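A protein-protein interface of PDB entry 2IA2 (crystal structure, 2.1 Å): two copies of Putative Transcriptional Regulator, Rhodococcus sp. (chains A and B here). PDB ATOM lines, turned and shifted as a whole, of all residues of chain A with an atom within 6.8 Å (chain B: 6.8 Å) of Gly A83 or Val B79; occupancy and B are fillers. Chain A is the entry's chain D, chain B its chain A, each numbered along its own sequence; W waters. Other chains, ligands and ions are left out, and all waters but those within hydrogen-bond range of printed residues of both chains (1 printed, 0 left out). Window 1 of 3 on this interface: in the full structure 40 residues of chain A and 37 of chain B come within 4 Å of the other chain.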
ATOM      1  N   ARG A  28      18.567  -8.503  18.571  1.00  0.00           N
ATOM      2  CA  ARG A  28      19.475  -9.163  17.646  1.00  0.00           C
ATOM      3  C   ARG A  28      20.747  -8.395  17.391  1.00  0.00           C
ATOM      4  O   ARG A  28      21.782  -8.995  17.116  1.00  0.00           O
ATOM      5  CB  ARG A  28      18.786  -9.294  16.297  1.00  0.00           C
ATOM      6  CG  ARG A  28      17.910 -10.487  16.200  1.00  0.00           C
ATOM      7  CD  ARG A  28      18.768 -11.714  16.153  1.00  0.00           C
ATOM      8  NE  ARG A  28      19.428 -11.857  14.860  1.00  0.00           N
ATOM      9  CZ  ARG A  28      19.073 -12.761  13.949  1.00  0.00           C
ATOM     10  NH1 ARG A  28      18.037 -13.585  14.195  1.00  0.00           N
ATOM     11  NH2 ARG A  28      19.751 -12.838  12.803  1.00  0.00           N
ATOM     12  N   ARG A  78      17.964 -12.810  31.465  1.00  0.00           N
ATOM     13  CA  ARG A  78      16.565 -13.227  31.186  1.00  0.00           C
ATOM     14  C   ARG A  78      16.383 -13.430  29.657  1.00  0.00           C
ATOM     15  O   ARG A  78      15.549 -14.197  29.250  1.00  0.00           O
ATOM     16  CB  ARG A  78      15.539 -12.229  31.781  1.00  0.00           C
ATOM     17  CG  ARG A  78      14.072 -12.544  31.444  1.00  0.00           C
ATOM     18  CD  ARG A  78      13.079 -11.453  32.039  1.00  0.00           C
ATOM     19  NE  ARG A  78      13.329 -11.164  33.459  1.00  0.00           N
ATOM     20  CZ  ARG A  78      12.402 -11.138  34.429  1.00  0.00           C
ATOM     21  NH1 ARG A  78      11.109 -11.393  34.183  1.00  0.00           N
ATOM     22  NH2 ARG A  78      12.757 -10.861  35.670  1.00  0.00           N
ATOM     23  N   VAL A  79      17.189 -12.771  28.834  1.00  0.00           N
ATOM     24  CA  VAL A  79      17.142 -13.005  27.346  1.00  0.00           C
ATOM     25  C   VAL A  79      17.413 -14.486  26.994  1.00  0.00           C
ATOM     26  O   VAL A  79      16.862 -15.002  25.994  1.00  0.00           O
ATOM     27  CB  VAL A  79      18.067 -12.070  26.565  1.00  0.00           C
ATOM     28  CG1 VAL A  79      18.235 -12.492  25.050  1.00  0.00           C
ATOM     29  CG2 VAL A  79      17.535 -10.585  26.657  1.00  0.00           C
ATOM     30  N   LEU A  80      18.201 -15.172  27.845  1.00  0.00           N
ATOM     31  CA  LEU A  80      18.458 -16.612  27.668  1.00  0.00           C
ATOM     32  C   LEU A  80      17.194 -17.437  27.742  1.00  0.00           C
ATOM     33  O   LEU A  80      17.155 -18.496  27.186  1.00  0.00           O
ATOM     34  CB  LEU A  80      19.453 -17.109  28.694  1.00  0.00           C
ATOM     35  CG  LEU A  80      20.871 -16.523  28.575  1.00  0.00           C
ATOM     36  CD1 LEU A  80      21.735 -16.811  29.842  1.00  0.00           C
ATOM     37  CD2 LEU A  80      21.572 -17.113  27.377  1.00  0.00           C
ATOM     38  N   GLU A  81      16.123 -16.943  28.377  1.00  0.00           N
ATOM     39  CA  GLU A  81      14.839 -17.734  28.379  1.00  0.00           C
ATOM     40  C   GLU A  81      14.205 -17.866  26.966  1.00  0.00           C
ATOM     41  O   GLU A  81      13.331 -18.730  26.717  1.00  0.00           O
ATOM     42  CB  GLU A  81      13.803 -17.080  29.341  1.00  0.00           C
ATOM     43  CG  GLU A  81      14.266 -16.795  30.781  1.00  0.00           C
ATOM     44  CD  GLU A  81      14.483 -18.102  31.579  1.00  0.00           C
ATOM     45  OE1 GLU A  81      14.388 -19.225  31.008  1.00  0.00           O
ATOM     46  OE2 GLU A  81      14.761 -18.020  32.799  1.00  0.00           O
ATOM     47  N   LEU A  82      14.586 -16.989  26.061  1.00  0.00           N
ATOM     48  CA  LEU A  82      14.002 -17.053  24.689  1.00  0.00           C
ATOM     49  C   LEU A  82      14.631 -18.227  23.964  1.00  0.00           C
ATOM     50  O   LEU A  82      13.934 -19.152  23.592  1.00  0.00           O
ATOM     51  CB  LEU A  82      14.244 -15.746  23.918  1.00  0.00           C
ATOM     52  CG  LEU A  82      13.486 -14.578  24.539  1.00  0.00           C
ATOM     53  CD1 LEU A  82      14.039 -13.271  23.946  1.00  0.00           C
ATOM     54  CD2 LEU A  82      11.947 -14.699  24.327  1.00  0.00           C
ATOM     55  N   GLY A  83      15.958 -18.189  23.803  1.00  0.00           N
ATOM     56  CA  GLY A  83      16.716 -19.358  23.299  1.00  0.00           C
ATOM     57  C   GLY A  83      16.393 -20.647  24.047  1.00  0.00           C
ATOM     58  O   GLY A  83      16.325 -21.682  23.416  1.00  0.00           O
ATOM     59  N   TYR A  84      16.188 -20.594  25.379  1.00  0.00           N
ATOM     60  CA  TYR A  84      15.981 -21.831  26.131  1.00  0.00           C
ATOM     61  C   TYR A  84      14.597 -22.434  25.854  1.00  0.00           C
ATOM     62  O   TYR A  84      14.398 -23.612  26.073  1.00  0.00           O
ATOM     63  CB  TYR A  84      16.162 -21.671  27.655  1.00  0.00           C
ATOM     64  CG  TYR A  84      16.364 -23.010  28.331  1.00  0.00           C
ATOM     65  CD1 TYR A  84      17.525 -23.736  28.114  1.00  0.00           C
ATOM     66  CD2 TYR A  84      15.409 -23.550  29.154  1.00  0.00           C
ATOM     67  CE1 TYR A  84      17.746 -24.979  28.714  1.00  0.00           C
ATOM     68  CE2 TYR A  84      15.604 -24.854  29.762  1.00  0.00           C
ATOM     69  CZ  TYR A  84      16.800 -25.527  29.517  1.00  0.00           C
ATOM     70  OH  TYR A  84      17.058 -26.797  30.078  1.00  0.00           O
ATOM     71  N   SER A  85      13.637 -21.622  25.421  1.00  0.00           N
ATOM     72  CA  SER A  85      12.302 -22.153  25.047  1.00  0.00           C
ATOM     73  C   SER A  85      12.473 -23.073  23.831  1.00  0.00           C
ATOM     74  O   SER A  85      11.870 -24.153  23.755  1.00  0.00           O
ATOM     75  CB  SER A  85      11.353 -20.978  24.720  1.00  0.00           C
ATOM     76  OG  SER A  85      11.160 -20.172  25.892  1.00  0.00           O
ATOM     77  N   TYR A  86      13.296 -22.639  22.883  1.00  0.00           N
ATOM     78  CA  TYR A  86      13.708 -23.493  21.775  1.00  0.00           C
ATOM     79  C   TYR A  86      14.398 -24.757  22.280  1.00  0.00           C
ATOM     80  O   TYR A  86      13.912 -25.868  22.064  1.00  0.00           O
ATOM     81  CB  TYR A  86      14.637 -22.732  20.827  1.00  0.00           C
ATOM     82  CG  TYR A  86      15.273 -23.599  19.763  1.00  0.00           C
ATOM     83  CD1 TYR A  86      14.505 -24.177  18.761  1.00  0.00           C
ATOM     84  CD2 TYR A  86      16.640 -23.840  19.761  1.00  0.00           C
ATOM     85  CE1 TYR A  86      15.080 -24.970  17.787  1.00  0.00           C
ATOM     86  CE2 TYR A  86      17.225 -24.632  18.792  1.00  0.00           C
ATOM     87  CZ  TYR A  86      16.440 -25.194  17.807  1.00  0.00           C
ATOM     88  OH  TYR A  86      17.018 -25.983  16.839  1.00  0.00           O
ATOM     89  N   LEU A  87      15.529 -24.580  22.953  1.00  0.00           N
ATOM     90  CA  LEU A  87      16.352 -25.706  23.377  1.00  0.00           C
ATOM     91  C   LEU A  87      15.531 -26.726  24.158  1.00  0.00           C
ATOM     92  O   LEU A  87      15.665 -27.933  23.954  1.00  0.00           O
ATOM     93  CB  LEU A  87      17.528 -25.219  24.226  1.00  0.00           C
ATOM     94  CG  LEU A  87      18.569 -24.355  23.511  1.00  0.00           C
ATOM     95  CD1 LEU A  87      19.578 -23.796  24.502  1.00  0.00           C
ATOM     96  CD2 LEU A  87      19.270 -25.150  22.418  1.00  0.00           C
ATOM     97  N   SER A  88      14.679 -26.234  25.051  1.00  0.00           N
ATOM     98  CA  SER A  88      13.957 -27.096  25.979  1.00  0.00           C
ATOM     99  C   SER A  88      12.797 -27.802  25.285  1.00  0.00           C
ATOM    100  O   SER A  88      12.386 -28.889  25.693  1.00  0.00           O
ATOM    101  CB  SER A  88      13.443 -26.289  27.173  1.00  0.00           C
ATOM    102  OG  SER A  88      12.475 -25.337  26.766  1.00  0.00           O
ATOM    103  N   ILE B  27       6.923 -16.710  22.161  1.00  0.00           N
ATOM    104  CA  ILE B  27       8.151 -17.514  22.046  1.00  0.00           C
ATOM    105  C   ILE B  27       8.339 -18.253  23.367  1.00  0.00           C
ATOM    106  O   ILE B  27       8.647 -19.450  23.350  1.00  0.00           O
ATOM    107  CB  ILE B  27       9.425 -16.619  21.812  1.00  0.00           C
ATOM    108  CG1 ILE B  27       9.385 -15.994  20.418  1.00  0.00           C
ATOM    109  CG2 ILE B  27      10.724 -17.422  22.027  1.00  0.00           C
ATOM    110  CD1 ILE B  27      10.487 -14.963  20.164  1.00  0.00           C
ATOM    111  N   GLY B  64      10.893 -16.258  10.662  1.00  0.00           N
ATOM    112  CA  GLY B  64      11.760 -17.451  10.699  1.00  0.00           C
ATOM    113  C   GLY B  64      12.069 -17.980  12.090  1.00  0.00           C
ATOM    114  O   GLY B  64      12.879 -18.924  12.245  1.00  0.00           O
ATOM    115  N   TYR B  65      11.371 -17.420  13.089  1.00  0.00           N
ATOM    116  CA  TYR B  65      11.515 -17.821  14.485  1.00  0.00           C
ATOM    117  C   TYR B  65      10.565 -18.959  14.831  1.00  0.00           C
ATOM    118  O   TYR B  65      10.823 -19.735  15.784  1.00  0.00           O
ATOM    119  CB  TYR B  65      11.228 -16.644  15.414  1.00  0.00           C
ATOM    120  CG  TYR B  65      12.316 -15.598  15.386  1.00  0.00           C
ATOM    121  CD1 TYR B  65      12.111 -14.366  14.807  1.00  0.00           C
ATOM    122  CD2 TYR B  65      13.548 -15.838  15.970  1.00  0.00           C
ATOM    123  CE1 TYR B  65      13.122 -13.377  14.789  1.00  0.00           C
ATOM    124  CE2 TYR B  65      14.566 -14.862  15.950  1.00  0.00           C
ATOM    125  CZ  TYR B  65      14.347 -13.646  15.360  1.00  0.00           C
ATOM    126  OH  TYR B  65      15.373 -12.711  15.330  1.00  0.00           O
ATOM    127  N   VAL B  66       9.484 -19.071  14.066  1.00  0.00           N
ATOM    128  CA  VAL B  66       8.476 -20.096  14.352  1.00  0.00           C
ATOM    129  C   VAL B  66       8.267 -20.815  13.058  1.00  0.00           C
ATOM    130  O   VAL B  66       8.384 -20.203  12.012  1.00  0.00           O
ATOM    131  CB  VAL B  66       7.134 -19.485  14.899  1.00  0.00           C
ATOM    132  CG1 VAL B  66       6.002 -20.465  14.879  1.00  0.00           C
ATOM    133  CG2 VAL B  66       7.292 -18.954  16.358  1.00  0.00           C
ATOM    134  N   LEU B  75       9.110 -23.702  17.663  1.00  0.00           N
ATOM    135  CA  LEU B  75      10.210 -22.772  17.457  1.00  0.00           C
ATOM    136  C   LEU B  75      11.272 -23.362  16.554  1.00  0.00           C
ATOM    137  O   LEU B  75      11.401 -24.564  16.446  1.00  0.00           O
ATOM    138  CB  LEU B  75      10.866 -22.354  18.779  1.00  0.00           C
ATOM    139  CG  LEU B  75       9.904 -21.631  19.730  1.00  0.00           C
ATOM    140  CD1 LEU B  75      10.583 -21.455  21.086  1.00  0.00           C
ATOM    141  CD2 LEU B  75       9.483 -20.289  19.112  1.00  0.00           C
ATOM    142  N   THR B  76      12.056 -22.488  15.943  1.00  0.00           N
ATOM    143  CA  THR B  76      13.151 -22.876  15.082  1.00  0.00           C
ATOM    144  C   THR B  76      14.428 -22.421  15.775  1.00  0.00           C
ATOM    145  O   THR B  76      14.356 -21.624  16.724  1.00  0.00           O
ATOM    146  CB  THR B  76      13.105 -22.113  13.738  1.00  0.00           C
ATOM    147  OG1 THR B  76      13.526 -20.769  13.964  1.00  0.00           O
ATOM    148  CG2 THR B  76      11.727 -22.147  13.040  1.00  0.00           C
ATOM    149  N   PRO B  77      15.611 -22.927  15.345  1.00  0.00           N
ATOM    150  CA  PRO B  77      16.907 -22.495  15.914  1.00  0.00           C
ATOM    151  C   PRO B  77      17.261 -21.047  15.711  1.00  0.00           C
ATOM    152  O   PRO B  77      18.250 -20.591  16.260  1.00  0.00           O
ATOM    153  CB  PRO B  77      17.949 -23.378  15.175  1.00  0.00           C
ATOM    154  CG  PRO B  77      17.204 -23.932  13.955  1.00  0.00           C
ATOM    155  CD  PRO B  77      15.757 -23.998  14.341  1.00  0.00           C
ATOM    156  N   ARG B  78      16.477 -20.287  14.943  1.00  0.00           N
ATOM    157  CA  ARG B  78      16.796 -18.864  14.809  1.00  0.00           C
ATOM    158  C   ARG B  78      16.648 -18.134  16.121  1.00  0.00           C
ATOM    159  O   ARG B  78      17.293 -17.105  16.358  1.00  0.00           O
ATOM    160  CB  ARG B  78      15.949 -18.218  13.716  1.00  0.00           C
ATOM    161  CG  ARG B  78      16.321 -16.707  13.430  1.00  0.00           C
ATOM    162  CD  ARG B  78      15.517 -16.112  12.263  1.00  0.00           C
ATOM    163  NE  ARG B  78      15.699 -16.983  11.126  1.00  0.00           N
ATOM    164  CZ  ARG B  78      16.284 -16.682   9.955  1.00  0.00           C
ATOM    165  NH1 ARG B  78      16.754 -15.471   9.684  1.00  0.00           N
ATOM    166  NH2 ARG B  78      16.395 -17.636   9.037  1.00  0.00           N
ATOM    167  N   VAL B  79      15.814 -18.680  17.008  1.00  0.00           N
ATOM    168  CA  VAL B  79      15.631 -18.088  18.332  1.00  0.00           C
ATOM    169  C   VAL B  79      16.937 -17.996  19.109  1.00  0.00           C
ATOM    170  O   VAL B  79      17.115 -17.087  19.886  1.00  0.00           O
ATOM    171  CB  VAL B  79      14.533 -18.909  19.137  1.00  0.00           C
ATOM    172  CG1 VAL B  79      14.130 -18.191  20.414  1.00  0.00           C
ATOM    173  CG2 VAL B  79      13.314 -19.119  18.198  1.00  0.00           C
ATOM    174  N   LEU B  80      17.865 -18.935  18.895  1.00  0.00           N
ATOM    175  CA  LEU B  80      19.213 -18.843  19.487  1.00  0.00           C
ATOM    176  C   LEU B  80      20.015 -17.620  19.077  1.00  0.00           C
ATOM    177  O   LEU B  80      20.928 -17.225  19.802  1.00  0.00           O
ATOM    178  CB  LEU B  80      20.057 -20.151  19.216  1.00  0.00           C
ATOM    179  CG  LEU B  80      19.446 -21.406  19.878  1.00  0.00           C
ATOM    180  CD1 LEU B  80      20.265 -22.678  19.446  1.00  0.00           C
ATOM    181  CD2 LEU B  80      19.457 -21.257  21.397  1.00  0.00           C
ATOM    182  N   GLU B  81      19.697 -17.036  17.922  1.00  0.00           N
ATOM    183  CA  GLU B  81      20.373 -15.827  17.493  1.00  0.00           C
ATOM    184  C   GLU B  81      20.092 -14.629  18.435  1.00  0.00           C
ATOM    185  O   GLU B  81      20.808 -13.611  18.432  1.00  0.00           O
ATOM    186  CB  GLU B  81      20.021 -15.562  16.003  1.00  0.00           C
ATOM    187  CG  GLU B  81      20.263 -16.904  15.131  1.00  0.00           C
ATOM    188  CD  GLU B  81      20.561 -16.777  13.598  1.00  0.00           C
ATOM    189  OE1 GLU B  81      21.167 -15.764  13.167  1.00  0.00           O
ATOM    190  OE2 GLU B  81      20.214 -17.732  12.833  1.00  0.00           O
ATOM    191  N   LEU B  82      19.058 -14.743  19.272  1.00  0.00           N
ATOM    192  CA  LEU B  82      18.739 -13.689  20.216  1.00  0.00           C
ATOM    193  C   LEU B  82      19.639 -13.822  21.457  1.00  0.00           C
ATOM    194  O   LEU B  82      19.173 -14.300  22.490  1.00  0.00           O
ATOM    195  CB  LEU B  82      17.243 -13.736  20.594  1.00  0.00           C
ATOM    196  CG  LEU B  82      16.188 -13.673  19.450  1.00  0.00           C
ATOM    197  CD1 LEU B  82      14.784 -14.215  19.858  1.00  0.00           C
ATOM    198  CD2 LEU B  82      16.072 -12.279  18.827  1.00  0.00           C
ATOM    199  N   GLY B  83      20.931 -13.507  21.336  1.00  0.00           N
ATOM    200  CA  GLY B  83      21.783 -13.326  22.532  1.00  0.00           C
ATOM    201  C   GLY B  83      22.485 -14.561  23.097  1.00  0.00           C
ATOM    202  O   GLY B  83      23.448 -14.439  23.899  1.00  0.00           O
ATOM    203  N   TYR B  84      22.113 -15.744  22.618  1.00  0.00           N
ATOM    204  CA  TYR B  84      22.421 -16.955  23.408  1.00  0.00           C
ATOM    205  C   TYR B  84      23.933 -17.227  23.513  1.00  0.00           C
ATOM    206  O   TYR B  84      24.427 -17.569  24.569  1.00  0.00           O
ATOM    207  CB  TYR B  84      21.647 -18.206  22.901  1.00  0.00           C
ATOM    208  CG  TYR B  84      21.351 -19.153  24.054  1.00  0.00           C
ATOM    209  CD1 TYR B  84      20.138 -19.069  24.774  1.00  0.00           C
ATOM    210  CD2 TYR B  84      22.324 -20.082  24.493  1.00  0.00           C
ATOM    211  CE1 TYR B  84      19.899 -19.950  25.895  1.00  0.00           C
ATOM    212  CE2 TYR B  84      22.095 -20.935  25.582  1.00  0.00           C
ATOM    213  CZ  TYR B  84      20.866 -20.854  26.265  1.00  0.00           C
ATOM    214  OH  TYR B  84      20.621 -21.708  27.330  1.00  0.00           O
HETATM  215  O   HOH W   1      18.036 -16.368  23.973  1.00  0.00           O
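OH of Tyr B65 sits at hydrogen-bond distance from NH1 of Arg A28 (3.0 Å). NH2 of Arg A28 lies within salt-bridge range of OE1 of Glu B81.
O of Gly B64 sits at hydrogen-bond distance from OG1 of Thr B76. O of Tyr B65 sits at hydrogen-bond distance from N of Thr B76 (3.0 Å). The side-chain hydroxyl (OG1) of Thr B76 sits close to the backbone NH (N) of Arg B78. O of Glu A81 lies within hydrogen-bond range of OG of Ser A85, at 2.7 Å. O of Tyr A84 sits at hydrogen-bond distance from OG of Ser A88 (2.7 Å). The side-chain hydroxyl (OG) of Ser A88 sits at hydrogen-bond distance from the backbone carbonyl oxygen (O) of Ser A85, 3.3 Å away.
Among the printed residues, pairs that only touch across the chains: Arg A28 with Arg B78 (3.6 Å), Arg A28 with Leu B82 (3.7 Å), Val A79 with Leu B82 (3.3 Å), Leu A80 with Tyr B84 (3.4 Å), Leu A82 with Ile B27 (3.8 Å), Leu A82 with Val B79 (3.3 Å), Gly A83 with Val B79 (3.9 Å), Gly A83 with Leu B80 (3.8 Å), Gly A83 with Tyr B84 (3.7 Å), Tyr A84 with Tyr B84 (3.8 Å), Ser A85 with Ile B27 (3.4 Å), Ser A85 with Leu B75 (3.7 Å), Tyr A86 with Leu B75 (3.5 Å), Tyr A86 with Thr B76 (3.3 Å), Tyr A86 with Pro B77 (3.2 Å), Tyr A86 with Leu B80 (3.7 Å), Leu A87 with Leu B80 (3.9 Å) and Leu A87 with Tyr B84 (3.7 Å).
Of the printed residues of chain A, Val B79 touches Leu A82 (3.3 Å) and Gly A83 (3.9 Å). Of the printed residues of chain A, Leu B75 touches Ser A85 (3.7 Å) and Tyr A86 (3.5 Å). Of the printed residues of chain A, Leu B80 touches Gly A83 (3.8 Å), Tyr A86 (3.7 Å) and Leu A87 (3.9 Å). Gly B83 touches none of the printed residues of chain A. The nearest residue of chain A that does not touch Val B79 is Tyr A86 (4.2 Å). The nearest printed residue of chain A that does not touch Arg B78 is Tyr A86 (5.7 Å).
Printed residues of chain B that touch a printed residue of chain A: Ile B27, Tyr B65, Leu B75, Thr B76, Pro B77, Arg B78, Val B79, Leu B80, Glu B81, Leu B82 and Tyr B84. Printed residues of chain A that touch a printed residue of chain B: Arg A28, Val A79, Leu A80, Leu A82, Gly A83, Tyr A84, Ser A85, Tyr A86 and Leu A87. Hydrophobic or aromatic side chains of chain A that line the printed part of chain B: Val A79, Leu A80, Leu A82, Tyr A84, Tyr A86 and Leu A87. Among the printed residues, 20 pairs touch across the chains.
Val A79 touches Leu B82, and with the chains exchanged Leu A82 touches Val B79. Leu A80 touches Tyr B84, but with the chains exchanged Tyr A84 does not touch Leu B80 (5.2 Å). Gly A83 touches Tyr B84, but with the chains exchanged Tyr A84 does not touch Gly B83 (9.0 Å). Tyr A84 touches its own counterpart, Tyr B84. 7 positions are printed for both chains.
Water W1 lies within hydrogen-bond range of the backbone carbonyl oxygen of Val A79 (2.7 Å), the backbone NH of Gly A83 (2.8 Å) and the backbone carbonyl oxygen of Leu B82 (2.8 Å).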
